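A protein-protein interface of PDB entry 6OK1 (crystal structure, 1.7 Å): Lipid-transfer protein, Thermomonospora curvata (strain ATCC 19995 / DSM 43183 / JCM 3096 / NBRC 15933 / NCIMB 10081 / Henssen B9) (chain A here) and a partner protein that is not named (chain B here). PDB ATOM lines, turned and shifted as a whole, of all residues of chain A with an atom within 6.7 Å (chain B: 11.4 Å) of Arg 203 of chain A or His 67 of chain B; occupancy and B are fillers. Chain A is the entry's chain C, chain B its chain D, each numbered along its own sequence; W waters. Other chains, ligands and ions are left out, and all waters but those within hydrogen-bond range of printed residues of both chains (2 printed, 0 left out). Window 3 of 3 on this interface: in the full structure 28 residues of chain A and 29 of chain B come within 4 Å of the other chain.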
ATOM      1  N   GLN A 150     -16.526 -12.869 -25.738  1.00  0.00           N
ATOM      2  CA  GLN A 150     -17.696 -12.004 -25.671  1.00  0.00           C
ATOM      3  C   GLN A 150     -18.854 -12.690 -24.963  1.00  0.00           C
ATOM      4  O   GLN A 150     -19.558 -12.061 -24.160  1.00  0.00           O
ATOM      5  CB  GLN A 150     -18.110 -11.575 -27.077  1.00  0.00           C
ATOM      6  CG  GLN A 150     -17.131 -10.628 -27.723  1.00  0.00           C
ATOM      7  CD  GLN A 150     -17.286 -10.590 -29.226  1.00  0.00           C
ATOM      8  OE1 GLN A 150     -18.088 -11.332 -29.782  1.00  0.00           O
ATOM      9  NE2 GLN A 150     -16.508  -9.732 -29.895  1.00  0.00           N
ATOM     10  N   ASP A 198       0.549  -5.770 -14.738  1.00  0.00           N
ATOM     11  CA  ASP A 198       0.619  -6.274 -16.109  1.00  0.00           C
ATOM     12  C   ASP A 198      -0.777  -6.588 -16.626  1.00  0.00           C
ATOM     13  O   ASP A 198      -1.119  -6.300 -17.778  1.00  0.00           O
ATOM     14  CB  ASP A 198       1.472  -7.555 -16.192  1.00  0.00           C
ATOM     15  CG  ASP A 198       2.932  -7.321 -15.945  1.00  0.00           C
ATOM     16  OD1 ASP A 198       3.430  -6.215 -16.224  1.00  0.00           O
ATOM     17  OD2 ASP A 198       3.592  -8.269 -15.472  1.00  0.00           O
ATOM     18  N   HIS A 199      -1.575  -7.245 -15.789  1.00  0.00           N
ATOM     19  CA  HIS A 199      -2.931  -7.600 -16.163  1.00  0.00           C
ATOM     20  C   HIS A 199      -3.745  -6.352 -16.481  1.00  0.00           C
ATOM     21  O   HIS A 199      -4.382  -6.261 -17.537  1.00  0.00           O
ATOM     22  CB  HIS A 199      -3.550  -8.397 -15.030  1.00  0.00           C
ATOM     23  CG  HIS A 199      -4.991  -8.689 -15.231  1.00  0.00           C
ATOM     24  ND1 HIS A 199      -5.983  -7.807 -14.864  1.00  0.00           N
ATOM     25  CD2 HIS A 199      -5.615  -9.757 -15.781  1.00  0.00           C
ATOM     26  CE1 HIS A 199      -7.160  -8.332 -15.153  1.00  0.00           C
ATOM     27  NE2 HIS A 199      -6.962  -9.515 -15.716  1.00  0.00           N
ATOM     28  N   GLN A 200      -3.702  -5.357 -15.602  1.00  0.00           N
ATOM     29  CA  GLN A 200      -4.495  -4.155 -15.837  1.00  0.00           C
ATOM     30  C   GLN A 200      -3.992  -3.360 -17.035  1.00  0.00           C
ATOM     31  O   GLN A 200      -4.774  -2.646 -17.673  1.00  0.00           O
ATOM     32  CB  GLN A 200      -4.490  -3.278 -14.590  1.00  0.00           C
ATOM     33  CG  GLN A 200      -5.225  -3.874 -13.405  1.00  0.00           C
ATOM     34  CD  GLN A 200      -6.694  -4.027 -13.683  1.00  0.00           C
ATOM     35  OE1 GLN A 200      -7.447  -3.056 -13.640  1.00  0.00           O
ATOM     36  NE2 GLN A 200      -7.111  -5.238 -14.008  1.00  0.00           N
ATOM     37  N   ASN A 201      -2.697  -3.449 -17.351  1.00  0.00           N
ATOM     38  CA  ASN A 201      -2.171  -2.747 -18.514  1.00  0.00           C
ATOM     39  C   ASN A 201      -2.446  -3.479 -19.817  1.00  0.00           C
ATOM     40  O   ASN A 201      -2.289  -2.891 -20.887  1.00  0.00           O
ATOM     41  CB  ASN A 201      -0.665  -2.540 -18.374  1.00  0.00           C
ATOM     42  CG  ASN A 201      -0.324  -1.494 -17.342  1.00  0.00           C
ATOM     43  OD1 ASN A 201      -1.157  -0.661 -16.990  1.00  0.00           O
ATOM     44  ND2 ASN A 201       0.895  -1.536 -16.840  1.00  0.00           N
ATOM     45  N   SER A 202      -2.818  -4.749 -19.767  1.00  0.00           N
ATOM     46  CA  SER A 202      -3.002  -5.465 -21.011  1.00  0.00           C
ATOM     47  C   SER A 202      -4.249  -4.942 -21.721  1.00  0.00           C
ATOM     48  O   SER A 202      -5.182  -4.439 -21.097  1.00  0.00           O
ATOM     49  CB  SER A 202      -3.084  -6.978 -20.780  1.00  0.00           C
ATOM     50  OG  SER A 202      -4.262  -7.346 -20.088  1.00  0.00           O
ATOM     51  N   ARG A 203      -4.240  -5.047 -23.042  1.00  0.00           N
ATOM     52  CA  ARG A 203      -5.241  -4.376 -23.859  1.00  0.00           C
ATOM     53  C   ARG A 203      -6.628  -4.958 -23.615  1.00  0.00           C
ATOM     54  O   ARG A 203      -6.780  -6.117 -23.237  1.00  0.00           O
ATOM     55  CB  ARG A 203      -4.896  -4.503 -25.347  1.00  0.00           C
ATOM     56  CG  ARG A 203      -5.060  -5.939 -25.872  1.00  0.00           C
ATOM     57  CD  ARG A 203      -4.412  -6.100 -27.243  1.00  0.00           C
ATOM     58  NE  ARG A 203      -4.951  -5.120 -28.170  1.00  0.00           N
ATOM     59  CZ  ARG A 203      -4.572  -5.005 -29.436  1.00  0.00           C
ATOM     60  NH1 ARG A 203      -3.653  -5.820 -29.916  1.00  0.00           N
ATOM     61  NH2 ARG A 203      -5.125  -4.087 -30.212  1.00  0.00           N
ATOM     62  N   TRP A 204      -7.652  -4.148 -23.864  1.00  0.00           N
ATOM     63  CA  TRP A 204      -9.018  -4.658 -23.827  1.00  0.00           C
ATOM     64  C   TRP A 204      -9.263  -5.626 -24.973  1.00  0.00           C
ATOM     65  O   TRP A 204      -8.903  -5.350 -26.121  1.00  0.00           O
ATOM     66  CB  TRP A 204     -10.022  -3.514 -23.924  1.00  0.00           C
ATOM     67  CG  TRP A 204     -10.113  -2.677 -22.724  1.00  0.00           C
ATOM     68  CD1 TRP A 204      -9.827  -1.355 -22.630  1.00  0.00           C
ATOM     69  CD2 TRP A 204     -10.542  -3.093 -21.426  1.00  0.00           C
ATOM     70  NE1 TRP A 204     -10.049  -0.913 -21.348  1.00  0.00           N
ATOM     71  CE2 TRP A 204     -10.484  -1.965 -20.586  1.00  0.00           C
ATOM     72  CE3 TRP A 204     -10.964  -4.317 -20.888  1.00  0.00           C
ATOM     73  CZ2 TRP A 204     -10.836  -2.014 -19.240  1.00  0.00           C
ATOM     74  CZ3 TRP A 204     -11.310  -4.370 -19.551  1.00  0.00           C
ATOM     75  CH2 TRP A 204     -11.253  -3.218 -18.739  1.00  0.00           C
ATOM     76  N   ILE A 205      -9.887  -6.767 -24.669  1.00  0.00           N
ATOM     77  CA  ILE A 205     -10.423  -7.624 -25.720  1.00  0.00           C
ATOM     78  C   ILE A 205     -11.898  -7.297 -25.866  1.00  0.00           C
ATOM     79  O   ILE A 205     -12.335  -6.769 -26.892  1.00  0.00           O
ATOM     80  CB  ILE A 205     -10.186  -9.111 -25.405  1.00  0.00           C
ATOM     81  CG1 ILE A 205      -8.680  -9.393 -25.321  1.00  0.00           C
ATOM     82  CG2 ILE A 205     -10.837  -9.997 -26.450  1.00  0.00           C
ATOM     83  CD1 ILE A 205      -7.912  -9.072 -26.592  1.00  0.00           C
ATOM     84  N   VAL A 206     -12.667  -7.574 -24.820  1.00  0.00           N
ATOM     85  CA  VAL A 206     -14.077  -7.225 -24.764  1.00  0.00           C
ATOM     86  C   VAL A 206     -14.356  -6.905 -23.303  1.00  0.00           C
ATOM     87  O   VAL A 206     -14.164  -7.761 -22.432  1.00  0.00           O
ATOM     88  CB  VAL A 206     -14.983  -8.353 -25.314  1.00  0.00           C
ATOM     89  CG1 VAL A 206     -14.545  -9.736 -24.806  1.00  0.00           C
ATOM     90  CG2 VAL A 206     -16.454  -8.112 -24.982  1.00  0.00           C
ATOM     91  N   LEU A 209     -13.126  -7.849 -20.027  1.00  0.00           N
ATOM     92  CA  LEU A 209     -12.006  -8.768 -20.148  1.00  0.00           C
ATOM     93  C   LEU A 209     -10.826  -8.112 -20.861  1.00  0.00           C
ATOM     94  O   LEU A 209     -10.954  -7.636 -21.996  1.00  0.00           O
ATOM     95  CB  LEU A 209     -12.432 -10.025 -20.903  1.00  0.00           C
ATOM     96  CG  LEU A 209     -13.172 -11.079 -20.089  1.00  0.00           C
ATOM     97  CD1 LEU A 209     -14.460 -10.562 -19.556  1.00  0.00           C
ATOM     98  CD2 LEU A 209     -13.435 -12.275 -20.934  1.00  0.00           C
ATOM     99  N   HIS A 210      -9.676  -8.135 -20.197  1.00  0.00           N
ATOM    100  CA  HIS A 210      -8.386  -7.822 -20.776  1.00  0.00           C
ATOM    101  C   HIS A 210      -7.813  -9.019 -21.518  1.00  0.00           C
ATOM    102  O   HIS A 210      -8.220 -10.167 -21.327  1.00  0.00           O
ATOM    103  CB  HIS A 210      -7.384  -7.466 -19.691  1.00  0.00           C
ATOM    104  CG  HIS A 210      -7.700  -6.210 -18.944  1.00  0.00           C
ATOM    105  ND1 HIS A 210      -7.058  -5.021 -19.204  1.00  0.00           N
ATOM    106  CD2 HIS A 210      -8.558  -5.965 -17.925  1.00  0.00           C
ATOM    107  CE1 HIS A 210      -7.517  -4.085 -18.383  1.00  0.00           C
ATOM    108  NE2 HIS A 210      -8.426  -4.632 -17.595  1.00  0.00           N
ATOM    109  N   LEU A 211      -6.758  -8.758 -22.287  1.00  0.00           N
ATOM    110  CA  LEU A 211      -6.066  -9.859 -22.959  1.00  0.00           C
ATOM    111  C   LEU A 211      -5.625 -10.933 -21.974  1.00  0.00           C
ATOM    112  O   LEU A 211      -5.757 -12.129 -22.255  1.00  0.00           O
ATOM    113  CB  LEU A 211      -4.857  -9.320 -23.718  1.00  0.00           C
ATOM    114  CG  LEU A 211      -3.957 -10.336 -24.430  1.00  0.00           C
ATOM    115  CD1 LEU A 211      -4.760 -11.155 -25.387  1.00  0.00           C
ATOM    116  CD2 LEU A 211      -2.836  -9.614 -25.157  1.00  0.00           C
ATOM    117  N   LEU A 212      -5.090 -10.535 -20.826  1.00  0.00           N
ATOM    118  CA  LEU A 212      -4.597 -11.525 -19.887  1.00  0.00           C
ATOM    119  C   LEU A 212      -5.711 -12.182 -19.078  1.00  0.00           C
ATOM    120  O   LEU A 212      -5.406 -13.026 -18.232  1.00  0.00           O
ATOM    121  CB  LEU A 212      -3.547 -10.893 -18.971  1.00  0.00           C
ATOM    122  CG  LEU A 212      -2.208 -10.615 -19.679  1.00  0.00           C
ATOM    123  CD1 LEU A 212      -1.266  -9.877 -18.756  1.00  0.00           C
ATOM    124  CD2 LEU A 212      -1.550 -11.900 -20.187  1.00  0.00           C
ATOM    125  N   ILE B  63     -21.638  -5.884 -23.284  1.00  0.00           N
ATOM    126  CA  ILE B  63     -20.213  -6.024 -23.547  1.00  0.00           C
ATOM    127  C   ILE B  63     -19.778  -4.915 -24.491  1.00  0.00           C
ATOM    128  O   ILE B  63     -20.569  -4.409 -25.290  1.00  0.00           O
ATOM    129  CB  ILE B  63     -19.880  -7.416 -24.140  1.00  0.00           C
ATOM    130  CG1 ILE B  63     -20.554  -7.631 -25.501  1.00  0.00           C
ATOM    131  CG2 ILE B  63     -20.324  -8.489 -23.172  1.00  0.00           C
ATOM    132  CD1 ILE B  63     -19.739  -7.240 -26.709  1.00  0.00           C
ATOM    133  N   VAL B  64     -18.488  -4.582 -24.440  1.00  0.00           N
ATOM    134  CA  VAL B  64     -17.883  -3.607 -25.345  1.00  0.00           C
ATOM    135  C   VAL B  64     -16.733  -4.318 -26.045  1.00  0.00           C
ATOM    136  O   VAL B  64     -15.722  -4.633 -25.414  1.00  0.00           O
ATOM    137  CB  VAL B  64     -17.394  -2.354 -24.605  1.00  0.00           C
ATOM    138  CG1 VAL B  64     -16.936  -1.287 -25.596  1.00  0.00           C
ATOM    139  CG2 VAL B  64     -18.489  -1.827 -23.685  1.00  0.00           C
ATOM    140  N   ALA B  65     -16.886  -4.559 -27.341  1.00  0.00           N
ATOM    141  CA  ALA B  65     -15.912  -5.317 -28.117  1.00  0.00           C
ATOM    142  C   ALA B  65     -14.850  -4.369 -28.663  1.00  0.00           C
ATOM    143  O   ALA B  65     -15.177  -3.425 -29.380  1.00  0.00           O
ATOM    144  CB  ALA B  65     -16.613  -6.050 -29.260  1.00  0.00           C
ATOM    145  N   HIS B  66     -13.584  -4.612 -28.326  1.00  0.00           N
ATOM    146  CA  HIS B  66     -12.495  -3.733 -28.761  1.00  0.00           C
ATOM    147  C   HIS B  66     -11.581  -4.349 -29.805  1.00  0.00           C
ATOM    148  O   HIS B  66     -11.131  -3.654 -30.723  1.00  0.00           O
ATOM    149  CB  HIS B  66     -11.641  -3.328 -27.565  1.00  0.00           C
ATOM    150  CG  HIS B  66     -12.305  -2.345 -26.659  1.00  0.00           C
ATOM    151  ND1 HIS B  66     -12.166  -0.986 -26.827  1.00  0.00           N
ATOM    152  CD2 HIS B  66     -13.117  -2.516 -25.591  1.00  0.00           C
ATOM    153  CE1 HIS B  66     -12.856  -0.360 -25.891  1.00  0.00           C
ATOM    154  NE2 HIS B  66     -13.439  -1.263 -25.126  1.00  0.00           N
ATOM    155  N   HIS B  67     -11.284  -5.634 -29.660  1.00  0.00           N
ATOM    156  CA  HIS B  67     -10.231  -6.289 -30.410  1.00  0.00           C
ATOM    157  C   HIS B  67     -10.457  -7.781 -30.279  1.00  0.00           C
ATOM    158  O   HIS B  67     -10.786  -8.245 -29.174  1.00  0.00           O
ATOM    159  CB  HIS B  67      -8.847  -5.921 -29.871  1.00  0.00           C
ATOM    160  CG  HIS B  67      -7.724  -6.561 -30.617  1.00  0.00           C
ATOM    161  ND1 HIS B  67      -7.190  -6.015 -31.762  1.00  0.00           N
ATOM    162  CD2 HIS B  67      -7.046  -7.712 -30.395  1.00  0.00           C
ATOM    163  CE1 HIS B  67      -6.221  -6.796 -32.210  1.00  0.00           C
ATOM    164  NE2 HIS B  67      -6.116  -7.835 -31.399  1.00  0.00           N
ATOM    165  N   PRO B  68     -10.289  -8.567 -31.353  1.00  0.00           N
ATOM    166  CA  PRO B  68      -9.856  -8.164 -32.697  1.00  0.00           C
ATOM    167  C   PRO B  68     -10.955  -7.503 -33.531  1.00  0.00           C
ATOM    168  O   PRO B  68     -12.120  -7.537 -33.146  1.00  0.00           O
ATOM    169  CB  PRO B  68      -9.435  -9.490 -33.330  1.00  0.00           C
ATOM    170  CG  PRO B  68     -10.286 -10.477 -32.694  1.00  0.00           C
ATOM    171  CD  PRO B  68     -10.522 -10.018 -31.276  1.00  0.00           C
ATOM    172  N   PRO B  69     -10.591  -6.919 -34.676  1.00  0.00           N
ATOM    173  CA  PRO B  69     -11.599  -6.229 -35.494  1.00  0.00           C
ATOM    174  C   PRO B  69     -12.652  -7.175 -36.057  1.00  0.00           C
ATOM    175  O   PRO B  69     -12.360  -8.301 -36.474  1.00  0.00           O
ATOM    176  CB  PRO B  69     -10.773  -5.589 -36.619  1.00  0.00           C
ATOM    177  CG  PRO B  69      -9.377  -5.574 -36.122  1.00  0.00           C
ATOM    178  CD  PRO B  69      -9.243  -6.780 -35.243  1.00  0.00           C
ATOM    179  N   HIS B  70     -13.895  -6.687 -36.063  1.00  0.00           N
ATOM    180  CA  HIS B  70     -15.034  -7.299 -36.734  1.00  0.00           C
ATOM    181  C   HIS B  70     -15.279  -6.573 -38.049  1.00  0.00           C
ATOM    182  O   HIS B  70     -15.334  -5.332 -38.058  1.00  0.00           O
ATOM    183  CB  HIS B  70     -16.283  -7.211 -35.860  1.00  0.00           C
ATOM    184  CG  HIS B  70     -17.409  -8.088 -36.312  1.00  0.00           C
ATOM    185  ND1 HIS B  70     -18.101  -7.871 -37.486  1.00  0.00           N
ATOM    186  CD2 HIS B  70     -17.972  -9.178 -35.740  1.00  0.00           C
ATOM    187  CE1 HIS B  70     -19.035  -8.795 -37.620  1.00  0.00           C
ATOM    188  NE2 HIS B  70     -18.979  -9.601 -36.573  1.00  0.00           N
ATOM    189  N   PRO B  71     -15.436  -7.274 -39.174  1.00  0.00           N
ATOM    190  CA  PRO B  71     -15.589  -6.554 -40.455  1.00  0.00           C
ATOM    191  C   PRO B  71     -16.855  -5.719 -40.563  1.00  0.00           C
ATOM    192  O   PRO B  71     -16.819  -4.617 -41.120  1.00  0.00           O
ATOM    193  CB  PRO B  71     -15.581  -7.682 -41.491  1.00  0.00           C
ATOM    194  CG  PRO B  71     -14.953  -8.840 -40.803  1.00  0.00           C
ATOM    195  CD  PRO B  71     -15.331  -8.728 -39.369  1.00  0.00           C
ATOM    196  N   PHE B  73     -18.529  -4.082 -38.394  1.00  0.00           N
ATOM    197  CA  PHE B  73     -18.753  -3.126 -37.322  1.00  0.00           C
ATOM    198  C   PHE B  73     -17.554  -2.201 -37.190  1.00  0.00           C
ATOM    199  O   PHE B  73     -16.409  -2.632 -37.348  1.00  0.00           O
ATOM    200  CB  PHE B  73     -18.990  -3.829 -35.974  1.00  0.00           C
ATOM    201  CG  PHE B  73     -20.316  -4.534 -35.861  1.00  0.00           C
ATOM    202  CD1 PHE B  73     -20.448  -5.857 -36.253  1.00  0.00           C
ATOM    203  CD2 PHE B  73     -21.419  -3.886 -35.324  1.00  0.00           C
ATOM    204  CE1 PHE B  73     -21.658  -6.512 -36.136  1.00  0.00           C
ATOM    205  CE2 PHE B  73     -22.630  -4.537 -35.206  1.00  0.00           C
ATOM    206  CZ  PHE B  73     -22.748  -5.852 -35.613  1.00  0.00           C
ATOM    207  N   GLU B  74     -17.837  -0.931 -36.901  1.00  0.00           N
ATOM    208  CA  GLU B  74     -16.806  -0.011 -36.444  1.00  0.00           C
ATOM    209  C   GLU B  74     -16.399  -0.388 -35.025  1.00  0.00           C
ATOM    210  O   GLU B  74     -17.256  -0.597 -34.165  1.00  0.00           O
ATOM    211  CB  GLU B  74     -17.322   1.427 -36.479  1.00  0.00           C
ATOM    212  CG  GLU B  74     -17.767   1.894 -37.850  1.00  0.00           C
ATOM    213  CD  GLU B  74     -16.622   1.960 -38.840  1.00  0.00           C
ATOM    214  OE1 GLU B  74     -15.454   1.871 -38.407  1.00  0.00           O
ATOM    215  OE2 GLU B  74     -16.888   2.099 -40.052  1.00  0.00           O
ATOM    216  N   MET B  75     -15.089  -0.484 -34.779  1.00  0.00           N
ATOM    217  CA  MET B  75     -14.634  -0.846 -33.437  1.00  0.00           C
ATOM    218  C   MET B  75     -14.412   0.407 -32.595  1.00  0.00           C
ATOM    219  O   MET B  75     -13.878   1.401 -33.094  1.00  0.00           O
ATOM    220  CB  MET B  75     -13.331  -1.644 -33.492  1.00  0.00           C
ATOM    221  CG  MET B  75     -13.387  -2.882 -34.365  1.00  0.00           C
ATOM    222  SD  MET B  75     -14.634  -4.088 -33.871  1.00  0.00           S
ATOM    223  CE  MET B  75     -13.942  -4.737 -32.334  1.00  0.00           C
ATOM    224  N   PRO B  76     -14.789   0.421 -31.307  1.00  0.00           N
ATOM    225  CA  PRO B  76     -15.490  -0.647 -30.579  1.00  0.00           C
ATOM    226  C   PRO B  76     -16.991  -0.616 -30.839  1.00  0.00           C
ATOM    227  O   PRO B  76     -17.507   0.407 -31.277  1.00  0.00           O
ATOM    228  CB  PRO B  76     -15.178  -0.329 -29.116  1.00  0.00           C
ATOM    229  CG  PRO B  76     -15.054   1.187 -29.097  1.00  0.00           C
ATOM    230  CD  PRO B  76     -14.426   1.550 -30.417  1.00  0.00           C
ATOM    231  N   TYR B  77     -17.693  -1.718 -30.593  1.00  0.00           N
ATOM    232  CA  TYR B  77     -19.145  -1.699 -30.665  1.00  0.00           C
ATOM    233  C   TYR B  77     -19.693  -2.382 -29.426  1.00  0.00           C
ATOM    234  O   TYR B  77     -18.953  -3.010 -28.670  1.00  0.00           O
ATOM    235  CB  TYR B  77     -19.658  -2.361 -31.945  1.00  0.00           C
ATOM    236  CG  TYR B  77     -19.305  -3.821 -32.093  1.00  0.00           C
ATOM    237  CD1 TYR B  77     -18.112  -4.201 -32.696  1.00  0.00           C
ATOM    238  CD2 TYR B  77     -20.176  -4.820 -31.663  1.00  0.00           C
ATOM    239  CE1 TYR B  77     -17.781  -5.531 -32.861  1.00  0.00           C
ATOM    240  CE2 TYR B  77     -19.864  -6.165 -31.835  1.00  0.00           C
ATOM    241  CZ  TYR B  77     -18.656  -6.514 -32.439  1.00  0.00           C
ATOM    242  OH  TYR B  77     -18.320  -7.846 -32.600  1.00  0.00           O
ATOM    243  N   VAL B  78     -20.995  -2.210 -29.203  1.00  0.00           N
ATOM    244  CA  VAL B  78     -21.660  -2.667 -27.991  1.00  0.00           C
ATOM    245  C   VAL B  78     -22.698  -3.701 -28.373  1.00  0.00           C
ATOM    246  O   VAL B  78     -23.480  -3.497 -29.308  1.00  0.00           O
ATOM    247  CB  VAL B  78     -22.313  -1.498 -27.225  1.00  0.00           C
ATOM    248  CG1 VAL B  78     -23.096  -2.017 -25.997  1.00  0.00           C
ATOM    249  CG2 VAL B  78     -21.252  -0.524 -26.789  1.00  0.00           C
HETATM  250  O   HOH W   1     -13.761  -8.587 -28.897  1.00  0.00           O
HETATM  251  O   HOH W   2     -16.088  -9.453 -32.853  1.00  0.00           O
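NH2 of Arg 203 of chain A lies within hydrogen-bond range of ND1 of His 67 of chain B, at 3.2 Å.
N of His 66 of chain B is in hydrogen-bond range of O of Ile 205 of chain A (2.9 Å).
The backbone carbonyl oxygen (O) of Ile 205 of chain A is in hydrogen-bond range of the backbone NH (N) of His 67 of chain B (3.2 Å).
The backbone carbonyl oxygen (O) of Arg 203 of chain A sits at hydrogen-bond distance from the backbone NH (N) of Leu 211 of chain A, 2.8 Å away.
The backbone carbonyl oxygen (O) of Tyr 77 of chain B lies within hydrogen-bond range of the backbone NH (N) of Ala 65 of chain B (2.9 Å).
Among the printed residues, pairs that only touch across the chains: Gln 150 of chain A with Ile 63 of chain B (3.8 Å), Gln 150 of chain A with Ala 65 of chain B (3.7 Å), Gln 150 of chain A with Tyr 77 of chain B (3.8 Å), Trp 204 of chain A with His 66 of chain B (3.7 Å), Trp 204 of chain A with His 67 of chain B (3.8 Å), Ile 205 of chain A with Ala 65 of chain B (3.9 Å), Val 206 of chain A with Ile 63 of chain B (3.6 Å) and Val 206 of chain A with Val 64 of chain B (3.1 Å).
Ser 202 of chain A touches none of the printed residues of chain B.
Arg 203 of chain A touches just one residue of chain B: His 67.
Of the printed residues of chain B, Trp 204 of chain A touches His 66 and His 67.
Of chain B, only Ala 65, His 66 and His 67 come within 4 Å of Ile 205 of chain A.
Of the printed residues of chain B, Val 206 of chain A touches Ile 63 (3.6 Å) and Val 64 (3.1 Å).
No residue of chain B comes within 4 Å of His 210 of chain A.
No residue of chain B comes within 4 Å of Leu 211 of chain A.
Printed residues of chain A within 4 Å of Val 64 of chain B: Val 206 (3.1 Å).
Printed residues of chain A within 4 Å of His 66 of chain B: Trp 204 and Ile 205.
Printed residues of chain A within 4 Å of His 67 of chain B: Arg 203, Trp 204 and Ile 205.
Phe 73 of chain B touches none of the printed residues of chain A.
Of the printed residues of chain A, Tyr 77 of chain B touches Gln 150.
The nearest residue of chain A that does not touch His 67 of chain B is Val 206 of chain A (4.8 Å).
Of the 14 printed residues of chain A, 5 touch a printed residue of chain B.
Hydrophobic or aromatic side chains of chain A that line the printed part of chain B: Trp 204, Ile 205 and Val 206.
Printed residues of chain B that touch a printed residue of chain A: Ile 63, Val 64, Ala 65, His 66, His 67 and Tyr 77.
Hydrophobic or aromatic side chains of chain B that line the printed part of chain A: Ile 63, Ala 65, His 66, His 67 and Tyr 77.
Among the printed residues, no Asp or Glu carboxylate lies within 4 Å of a Lys or Arg side-chain nitrogen of the other chain.
Water W2 bridges OH of Tyr 77 of chain B and NE2 of Gln 150 of chain A.
Water W1 lies within hydrogen-bond range of O of His 67 of chain B (3.0 Å), O of Ile 205 of chain A (3.1 Å) and NE2 of Gln 150 of chain A (3.1 Å).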
